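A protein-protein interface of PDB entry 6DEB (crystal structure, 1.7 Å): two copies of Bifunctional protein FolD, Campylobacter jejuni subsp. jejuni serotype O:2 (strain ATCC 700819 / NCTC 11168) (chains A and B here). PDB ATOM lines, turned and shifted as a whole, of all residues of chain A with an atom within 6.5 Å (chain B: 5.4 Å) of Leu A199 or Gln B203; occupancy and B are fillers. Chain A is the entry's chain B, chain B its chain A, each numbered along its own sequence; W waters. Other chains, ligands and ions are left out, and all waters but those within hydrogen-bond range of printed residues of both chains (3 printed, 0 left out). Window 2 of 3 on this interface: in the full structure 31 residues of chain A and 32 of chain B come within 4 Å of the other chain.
The backbone carbonyl oxygen (O) of Asp B162 is in hydrogen-bond range of the backbone NH (N) of Asp B205, at 2.8 Å.
NZ of Lys B223 is in hydrogen-bond range of O of Gln B203, 3.4 Å away.
NZ of Lys B223 is in salt-bridge range of OD1 of Asp B205 (2.9 Å).
The side-chain carboxylate of Asp A196 sits at hydrogen-bond distance from the backbone NH of Leu A199.
Water W1 bridges OD1 of Asp B162 (2.6 Å) and N of Lys A195 (3.0 Å).
Water W2 lies within hydrogen-bond range of the side-chain hydroxyl (OH) of Tyr B200 (2.7 Å) and the side-chain hydroxyl (OG) of Ser A188 (2.9 Å).
Water W3 bridges the backbone NH (N) of Asp A196 (2.9 Å) and the side-chain carboxylate (OD1) of Asp B162 (3.0 Å).
Of the 11 printed residues of chain A, 4 touch a printed residue of chain B.
Printed residues of chain A that touch a printed residue of chain B: Ser A188, Lys A195, Leu A199 and Tyr A200.
Hydrophobic or aromatic side chains of chain A within 4 Å of the printed part of chain B: Leu A199 and Tyr A200.
Hydrophobic or aromatic side chains of chain B within 4 Å of the printed part of chain A: Tyr B200.
Leu A199 touches Gln B203, but with the chains exchanged Gln A203 does not touch Leu B199 (4.2 Å).
Tyr A200 touches Gln B203, but with the chains exchanged Gln A203 does not touch Tyr B200 (6.2 Å).
7 positions are printed for both chains.
NZ of Lys A195 lies within salt-bridge range of OD2 of Asp B205, at 2.8 Å.
NZ of Lys A195 is in salt-bridge range of OD2 of Asp B162, 3.8 Å away.
The side-chain hydroxyl of Tyr A200 lies within hydrogen-bond range of the side-chain carboxylate of Asp B162.
OG of Ser A188 touches CE1 of Tyr B200 (3.6 Å).
Gln B203 touches Leu A199.
Gln B203 touches Tyr A200 (OE1 to CE1, 3.999 Å).
Leu A199 touches just one residue of chain B: Gln B203.
Printed residues of chain A within 4 Å of Gln B203: Leu A199 (3.5 Å) and Tyr A200 (3.999 Å).
Of the printed residues of chain B, Ser A188 touches Tyr B200.
Printed residues of chain B within 4 Å of Tyr A200: Asp B162 (2.7 Å) and Gln B203 (3.999 Å).
Of the printed residues of chain A, Asp B205 touches Lys A195 (2.8 Å).
Lys B223 touches none of the printed residues of chain A.
Leu A197 touches none of the printed residues of chain B.
The nearest printed residue of chain A that does not touch Gln B203 is Gln A203 (5.6 Å).
The nearest printed residue of chain B that does not touch Ser A188 is Gln B203 (6.1 Å).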
ATOM      1  N   SER A 188     -27.093  21.034 -22.218  1.00  0.00           N
ATOM      2  CA  SER A 188     -27.050  19.588 -22.441  1.00  0.00           C
ATOM      3  C   SER A 188     -28.483  19.137 -22.687  1.00  0.00           C
ATOM      4  O   SER A 188     -29.387  19.535 -21.960  1.00  0.00           O
ATOM      5  CB  SER A 188     -26.515  18.845 -21.215  1.00  0.00           C
ATOM      6  OG  SER A 188     -25.150  19.154 -20.920  1.00  0.00           O
ATOM      7  N   LYS A 195     -27.311   7.699 -20.741  1.00  0.00           N
ATOM      8  CA  LYS A 195     -26.862   6.614 -19.880  1.00  0.00           C
ATOM      9  C   LYS A 195     -27.092   6.913 -18.409  1.00  0.00           C
ATOM     10  O   LYS A 195     -27.527   6.036 -17.653  1.00  0.00           O
ATOM     11  CB  LYS A 195     -25.386   6.311 -20.135  1.00  0.00           C
ATOM     12  CG  LYS A 195     -25.154   5.663 -21.501  1.00  0.00           C
ATOM     13  CD  LYS A 195     -23.714   5.207 -21.708  1.00  0.00           C
ATOM     14  CE  LYS A 195     -22.784   6.376 -21.820  1.00  0.00           C
ATOM     15  NZ  LYS A 195     -21.423   5.927 -22.238  1.00  0.00           N
ATOM     16  N   ASP A 196     -26.818   8.150 -18.010  1.00  0.00           N
ATOM     17  CA  ASP A 196     -26.915   8.531 -16.600  1.00  0.00           C
ATOM     18  C   ASP A 196     -27.374   9.983 -16.510  1.00  0.00           C
ATOM     19  O   ASP A 196     -26.573  10.901 -16.693  1.00  0.00           O
ATOM     20  CB  ASP A 196     -25.548   8.342 -15.942  1.00  0.00           C
ATOM     21  CG  ASP A 196     -25.513   8.814 -14.484  1.00  0.00           C
ATOM     22  OD1 ASP A 196     -24.400   8.885 -13.924  1.00  0.00           O
ATOM     23  OD2 ASP A 196     -26.581   9.118 -13.907  1.00  0.00           O
ATOM     24  N   LEU A 197     -28.660  10.199 -16.258  1.00  0.00           N
ATOM     25  CA  LEU A 197     -29.175  11.566 -16.226  1.00  0.00           C
ATOM     26  C   LEU A 197     -28.489  12.353 -15.119  1.00  0.00           C
ATOM     27  O   LEU A 197     -28.216  13.540 -15.287  1.00  0.00           O
ATOM     28  CB  LEU A 197     -30.691  11.628 -15.975  1.00  0.00           C
ATOM     29  CG  LEU A 197     -31.677  11.170 -17.039  1.00  0.00           C
ATOM     30  CD1 LEU A 197     -33.091  11.193 -16.461  1.00  0.00           C
ATOM     31  CD2 LEU A 197     -31.574  12.076 -18.243  1.00  0.00           C
ATOM     32  N   SER A 198     -28.225  11.689 -13.996  1.00  0.00           N
ATOM     33  CA  SER A 198     -27.692  12.373 -12.825  1.00  0.00           C
ATOM     34  C   SER A 198     -26.325  12.979 -13.079  1.00  0.00           C
ATOM     35  O   SER A 198     -25.973  13.974 -12.458  1.00  0.00           O
ATOM     36  CB  SER A 198     -27.621  11.439 -11.617  1.00  0.00           C
ATOM     37  OG  SER A 198     -28.921  11.122 -11.173  1.00  0.00           O
ATOM     38  N   LEU A 199     -25.554  12.375 -13.980  1.00  0.00           N
ATOM     39  CA  LEU A 199     -24.251  12.925 -14.361  1.00  0.00           C
ATOM     40  C   LEU A 199     -24.396  14.384 -14.786  1.00  0.00           C
ATOM     41  O   LEU A 199     -23.561  15.231 -14.432  1.00  0.00           O
ATOM     42  CB  LEU A 199     -23.598  12.097 -15.485  1.00  0.00           C
ATOM     43  CG  LEU A 199     -22.185  12.472 -15.975  1.00  0.00           C
ATOM     44  CD1 LEU A 199     -21.126  12.156 -14.933  1.00  0.00           C
ATOM     45  CD2 LEU A 199     -21.835  11.796 -17.311  1.00  0.00           C
ATOM     46  N   TYR A 200     -25.478  14.678 -15.513  1.00  0.00           N
ATOM     47  CA  TYR A 200     -25.728  16.011 -16.027  1.00  0.00           C
ATOM     48  C   TYR A 200     -26.449  16.888 -15.002  1.00  0.00           C
ATOM     49  O   TYR A 200     -26.059  18.053 -14.755  1.00  0.00           O
ATOM     50  CB  TYR A 200     -26.566  15.923 -17.308  1.00  0.00           C
ATOM     51  CG  TYR A 200     -25.793  15.296 -18.447  1.00  0.00           C
ATOM     52  CD1 TYR A 200     -24.977  16.081 -19.268  1.00  0.00           C
ATOM     53  CD2 TYR A 200     -25.859  13.938 -18.698  1.00  0.00           C
ATOM     54  CE1 TYR A 200     -24.252  15.518 -20.309  1.00  0.00           C
ATOM     55  CE2 TYR A 200     -25.131  13.365 -19.746  1.00  0.00           C
ATOM     56  CZ  TYR A 200     -24.331  14.158 -20.542  1.00  0.00           C
ATOM     57  OH  TYR A 200     -23.608  13.586 -21.580  1.00  0.00           O
ATOM     58  N   THR A 201     -27.493  16.328 -14.399  1.00  0.00           N
ATOM     59  CA  THR A 201     -28.345  17.119 -13.528  1.00  0.00           C
ATOM     60  C   THR A 201     -27.631  17.538 -12.255  1.00  0.00           C
ATOM     61  O   THR A 201     -27.893  18.627 -11.745  1.00  0.00           O
ATOM     62  CB  THR A 201     -29.687  16.415 -13.188  1.00  0.00           C
ATOM     63  OG1 THR A 201     -29.425  15.175 -12.528  1.00  0.00           O
ATOM     64  CG2 THR A 201     -30.502  16.136 -14.461  1.00  0.00           C
ATOM     65  N   ARG A 202     -26.727  16.698 -11.745  1.00  0.00           N
ATOM     66  CA  ARG A 202     -26.050  17.031 -10.493  1.00  0.00           C
ATOM     67  C   ARG A 202     -25.140  18.260 -10.579  1.00  0.00           C
ATOM     68  O   ARG A 202     -24.803  18.843  -9.548  1.00  0.00           O
ATOM     69  CB  ARG A 202     -25.269  15.834  -9.924  1.00  0.00           C
ATOM     70  CG  ARG A 202     -26.157  14.837  -9.233  1.00  0.00           C
ATOM     71  CD  ARG A 202     -25.384  13.600  -8.792  1.00  0.00           C
ATOM     72  NE  ARG A 202     -26.285  12.596  -8.233  1.00  0.00           N
ATOM     73  CZ  ARG A 202     -26.045  11.285  -8.241  1.00  0.00           C
ATOM     74  NH1 ARG A 202     -24.932  10.820  -8.794  1.00  0.00           N
ATOM     75  NH2 ARG A 202     -26.918  10.438  -7.699  1.00  0.00           N
ATOM     76  N   GLN A 203     -24.763  18.642 -11.798  1.00  0.00           N
ATOM     77  CA  GLN A 203     -23.895  19.797 -12.012  1.00  0.00           C
ATOM     78  C   GLN A 203     -24.692  21.016 -12.494  1.00  0.00           C
ATOM     79  O   GLN A 203     -24.125  22.109 -12.623  1.00  0.00           O
ATOM     80  CB  GLN A 203     -22.816  19.468 -13.045  1.00  0.00           C
ATOM     81  CG  GLN A 203     -21.999  18.254 -12.683  1.00  0.00           C
ATOM     82  CD  GLN A 203     -21.352  18.407 -11.325  1.00  0.00           C
ATOM     83  OE1 GLN A 203     -20.938  19.504 -10.946  1.00  0.00           O
ATOM     84  NE2 GLN A 203     -21.275  17.309 -10.576  1.00  0.00           N
ATOM     85  N   ALA A 204     -25.992  20.832 -12.750  1.00  0.00           N
ATOM     86  CA  ALA A 204     -26.789  21.871 -13.426  1.00  0.00           C
ATOM     87  C   ALA A 204     -27.138  23.086 -12.558  1.00  0.00           C
ATOM     88  O   ALA A 204     -27.522  22.940 -11.406  1.00  0.00           O
ATOM     89  CB  ALA A 204     -28.072  21.275 -13.979  1.00  0.00           C
ATOM     90  N   ASP B 162     -22.290   9.969 -24.726  1.00  0.00           N
ATOM     91  CA  ASP B 162     -22.227  11.306 -24.154  1.00  0.00           C
ATOM     92  C   ASP B 162     -21.321  12.131 -25.048  1.00  0.00           C
ATOM     93  O   ASP B 162     -20.104  11.909 -25.076  1.00  0.00           O
ATOM     94  CB  ASP B 162     -21.652  11.246 -22.734  1.00  0.00           C
ATOM     95  CG  ASP B 162     -22.571  10.520 -21.768  1.00  0.00           C
ATOM     96  OD1 ASP B 162     -23.742  10.926 -21.666  1.00  0.00           O
ATOM     97  OD2 ASP B 162     -22.137   9.535 -21.118  1.00  0.00           O
ATOM     98  N   SER B 198     -13.664  21.596 -19.244  1.00  0.00           N
ATOM     99  CA  SER B 198     -13.140  20.284 -18.880  1.00  0.00           C
ATOM    100  C   SER B 198     -14.123  19.433 -18.075  1.00  0.00           C
ATOM    101  O   SER B 198     -14.039  18.212 -18.105  1.00  0.00           O
ATOM    102  CB  SER B 198     -11.804  20.407 -18.139  1.00  0.00           C
ATOM    103  OG  SER B 198     -11.960  21.052 -16.888  1.00  0.00           O
ATOM    104  N   LEU B 199     -15.038  20.070 -17.345  1.00  0.00           N
ATOM    105  CA  LEU B 199     -16.106  19.335 -16.663  1.00  0.00           C
ATOM    106  C   LEU B 199     -16.890  18.490 -17.666  1.00  0.00           C
ATOM    107  O   LEU B 199     -17.254  17.351 -17.381  1.00  0.00           O
ATOM    108  CB  LEU B 199     -17.072  20.294 -15.960  1.00  0.00           C
ATOM    109  CG  LEU B 199     -18.284  19.682 -15.244  1.00  0.00           C
ATOM    110  CD1 LEU B 199     -17.833  18.756 -14.125  1.00  0.00           C
ATOM    111  CD2 LEU B 199     -19.207  20.774 -14.692  1.00  0.00           C
ATOM    112  N   TYR B 200     -17.125  19.050 -18.849  1.00  0.00           N
ATOM    113  CA  TYR B 200     -17.880  18.361 -19.878  1.00  0.00           C
ATOM    114  C   TYR B 200     -17.014  17.361 -20.658  1.00  0.00           C
ATOM    115  O   TYR B 200     -17.434  16.240 -20.948  1.00  0.00           O
ATOM    116  CB  TYR B 200     -18.483  19.373 -20.853  1.00  0.00           C
ATOM    117  CG  TYR B 200     -19.617  20.168 -20.268  1.00  0.00           C
ATOM    118  CD1 TYR B 200     -20.932  19.728 -20.395  1.00  0.00           C
ATOM    119  CD2 TYR B 200     -19.381  21.369 -19.604  1.00  0.00           C
ATOM    120  CE1 TYR B 200     -21.973  20.447 -19.857  1.00  0.00           C
ATOM    121  CE2 TYR B 200     -20.436  22.115 -19.059  1.00  0.00           C
ATOM    122  CZ  TYR B 200     -21.733  21.633 -19.208  1.00  0.00           C
ATOM    123  OH  TYR B 200     -22.785  22.339 -18.684  1.00  0.00           O
ATOM    124  N   THR B 201     -15.808  17.779 -21.017  1.00  0.00           N
ATOM    125  CA  THR B 201     -14.985  16.931 -21.873  1.00  0.00           C
ATOM    126  C   THR B 201     -14.496  15.687 -21.126  1.00  0.00           C
ATOM    127  O   THR B 201     -14.391  14.605 -21.715  1.00  0.00           O
ATOM    128  CB  THR B 201     -13.789  17.690 -22.477  1.00  0.00           C
ATOM    129  OG1 THR B 201     -12.978  18.230 -21.424  1.00  0.00           O
ATOM    130  CG2 THR B 201     -14.292  18.805 -23.368  1.00  0.00           C
ATOM    131  N   ARG B 202     -14.223  15.824 -19.834  1.00  0.00           N
ATOM    132  CA  ARG B 202     -13.693  14.691 -19.067  1.00  0.00           C
ATOM    133  C   ARG B 202     -14.651  13.501 -19.000  1.00  0.00           C
ATOM    134  O   ARG B 202     -14.215  12.370 -18.788  1.00  0.00           O
ATOM    135  CB  ARG B 202     -13.268  15.114 -17.660  1.00  0.00           C
ATOM    136  CG  ARG B 202     -11.946  15.882 -17.633  1.00  0.00           C
ATOM    137  CD  ARG B 202     -11.427  16.051 -16.198  1.00  0.00           C
ATOM    138  NE  ARG B 202     -12.518  16.404 -15.295  1.00  0.00           N
ATOM    139  CZ  ARG B 202     -12.730  17.627 -14.821  1.00  0.00           C
ATOM    140  NH1 ARG B 202     -11.907  18.618 -15.146  1.00  0.00           N
ATOM    141  NH2 ARG B 202     -13.758  17.855 -14.010  1.00  0.00           N
ATOM    142  N   GLN B 203     -15.945  13.764 -19.193  1.00  0.00           N
ATOM    143  CA  GLN B 203     -16.968  12.719 -19.112  1.00  0.00           C
ATOM    144  C   GLN B 203     -17.404  12.227 -20.496  1.00  0.00           C
ATOM    145  O   GLN B 203     -18.180  11.279 -20.604  1.00  0.00           O
ATOM    146  CB  GLN B 203     -18.193  13.196 -18.295  1.00  0.00           C
ATOM    147  CG  GLN B 203     -18.761  14.541 -18.741  1.00  0.00           C
ATOM    148  CD  GLN B 203     -19.851  15.105 -17.811  1.00  0.00           C
ATOM    149  OE1 GLN B 203     -20.819  15.735 -18.270  1.00  0.00           O
ATOM    150  NE2 GLN B 203     -19.687  14.892 -16.508  1.00  0.00           N
ATOM    151  N   ALA B 204     -16.889  12.854 -21.549  1.00  0.00           N
ATOM    152  CA  ALA B 204     -17.402  12.591 -22.894  1.00  0.00           C
ATOM    153  C   ALA B 204     -16.949  11.260 -23.506  1.00  0.00           C
ATOM    154  O   ALA B 204     -15.787  10.872 -23.392  1.00  0.00           O
ATOM    155  CB  ALA B 204     -17.013  13.736 -23.826  1.00  0.00           C
ATOM    156  N   ASP B 205     -17.866  10.578 -24.186  1.00  0.00           N
ATOM    157  CA  ASP B 205     -17.486   9.474 -25.067  1.00  0.00           C
ATOM    158  C   ASP B 205     -17.028   9.960 -26.436  1.00  0.00           C
ATOM    159  O   ASP B 205     -16.298   9.256 -27.133  1.00  0.00           O
ATOM    160  CB  ASP B 205     -18.673   8.544 -25.303  1.00  0.00           C
ATOM    161  CG  ASP B 205     -19.160   7.920 -24.043  1.00  0.00           C
ATOM    162  OD1 ASP B 205     -18.316   7.375 -23.300  1.00  0.00           O
ATOM    163  OD2 ASP B 205     -20.379   7.980 -23.784  1.00  0.00           O
ATOM    164  N   MET B 221      -7.998  16.572 -20.291  1.00  0.00           N
ATOM    165  CA  MET B 221      -9.403  16.961 -20.444  1.00  0.00           C
ATOM    166  C   MET B 221     -10.269  15.835 -20.952  1.00  0.00           C
ATOM    167  O   MET B 221     -11.466  16.011 -21.103  1.00  0.00           O
ATOM    168  CB  MET B 221      -9.529  18.165 -21.374  1.00  0.00           C
ATOM    169  CG  MET B 221      -8.833  19.398 -20.829  1.00  0.00           C
ATOM    170  SD  MET B 221      -8.608  20.706 -22.058  1.00  0.00           S
ATOM    171  CE  MET B 221     -10.294  21.214 -22.378  1.00  0.00           C
ATOM    172  N   LYS B 223     -11.168  11.332 -21.166  1.00  0.00           N
ATOM    173  CA  LYS B 223     -11.040  10.038 -20.523  1.00  0.00           C
ATOM    174  C   LYS B 223     -10.525   9.013 -21.530  1.00  0.00           C
ATOM    175  O   LYS B 223     -10.659   9.198 -22.747  1.00  0.00           O
ATOM    176  CB  LYS B 223     -12.385   9.568 -19.959  1.00  0.00           C
ATOM    177  CG  LYS B 223     -13.390   9.133 -21.017  1.00  0.00           C
ATOM    178  CD  LYS B 223     -14.718   8.769 -20.350  1.00  0.00           C
ATOM    179  CE  LYS B 223     -15.725   8.285 -21.373  1.00  0.00           C
ATOM    180  NZ  LYS B 223     -17.068   8.103 -20.765  1.00  0.00           N
HETATM  181  O   HOH W   1     -25.674   9.410 -22.612  1.00  0.00           O
HETATM  182  O   HOH W   2     -25.335  21.386 -19.052  1.00  0.00           O
HETATM  183  O   HOH W   3     -24.733   9.888 -19.013  1.00  0.00           O
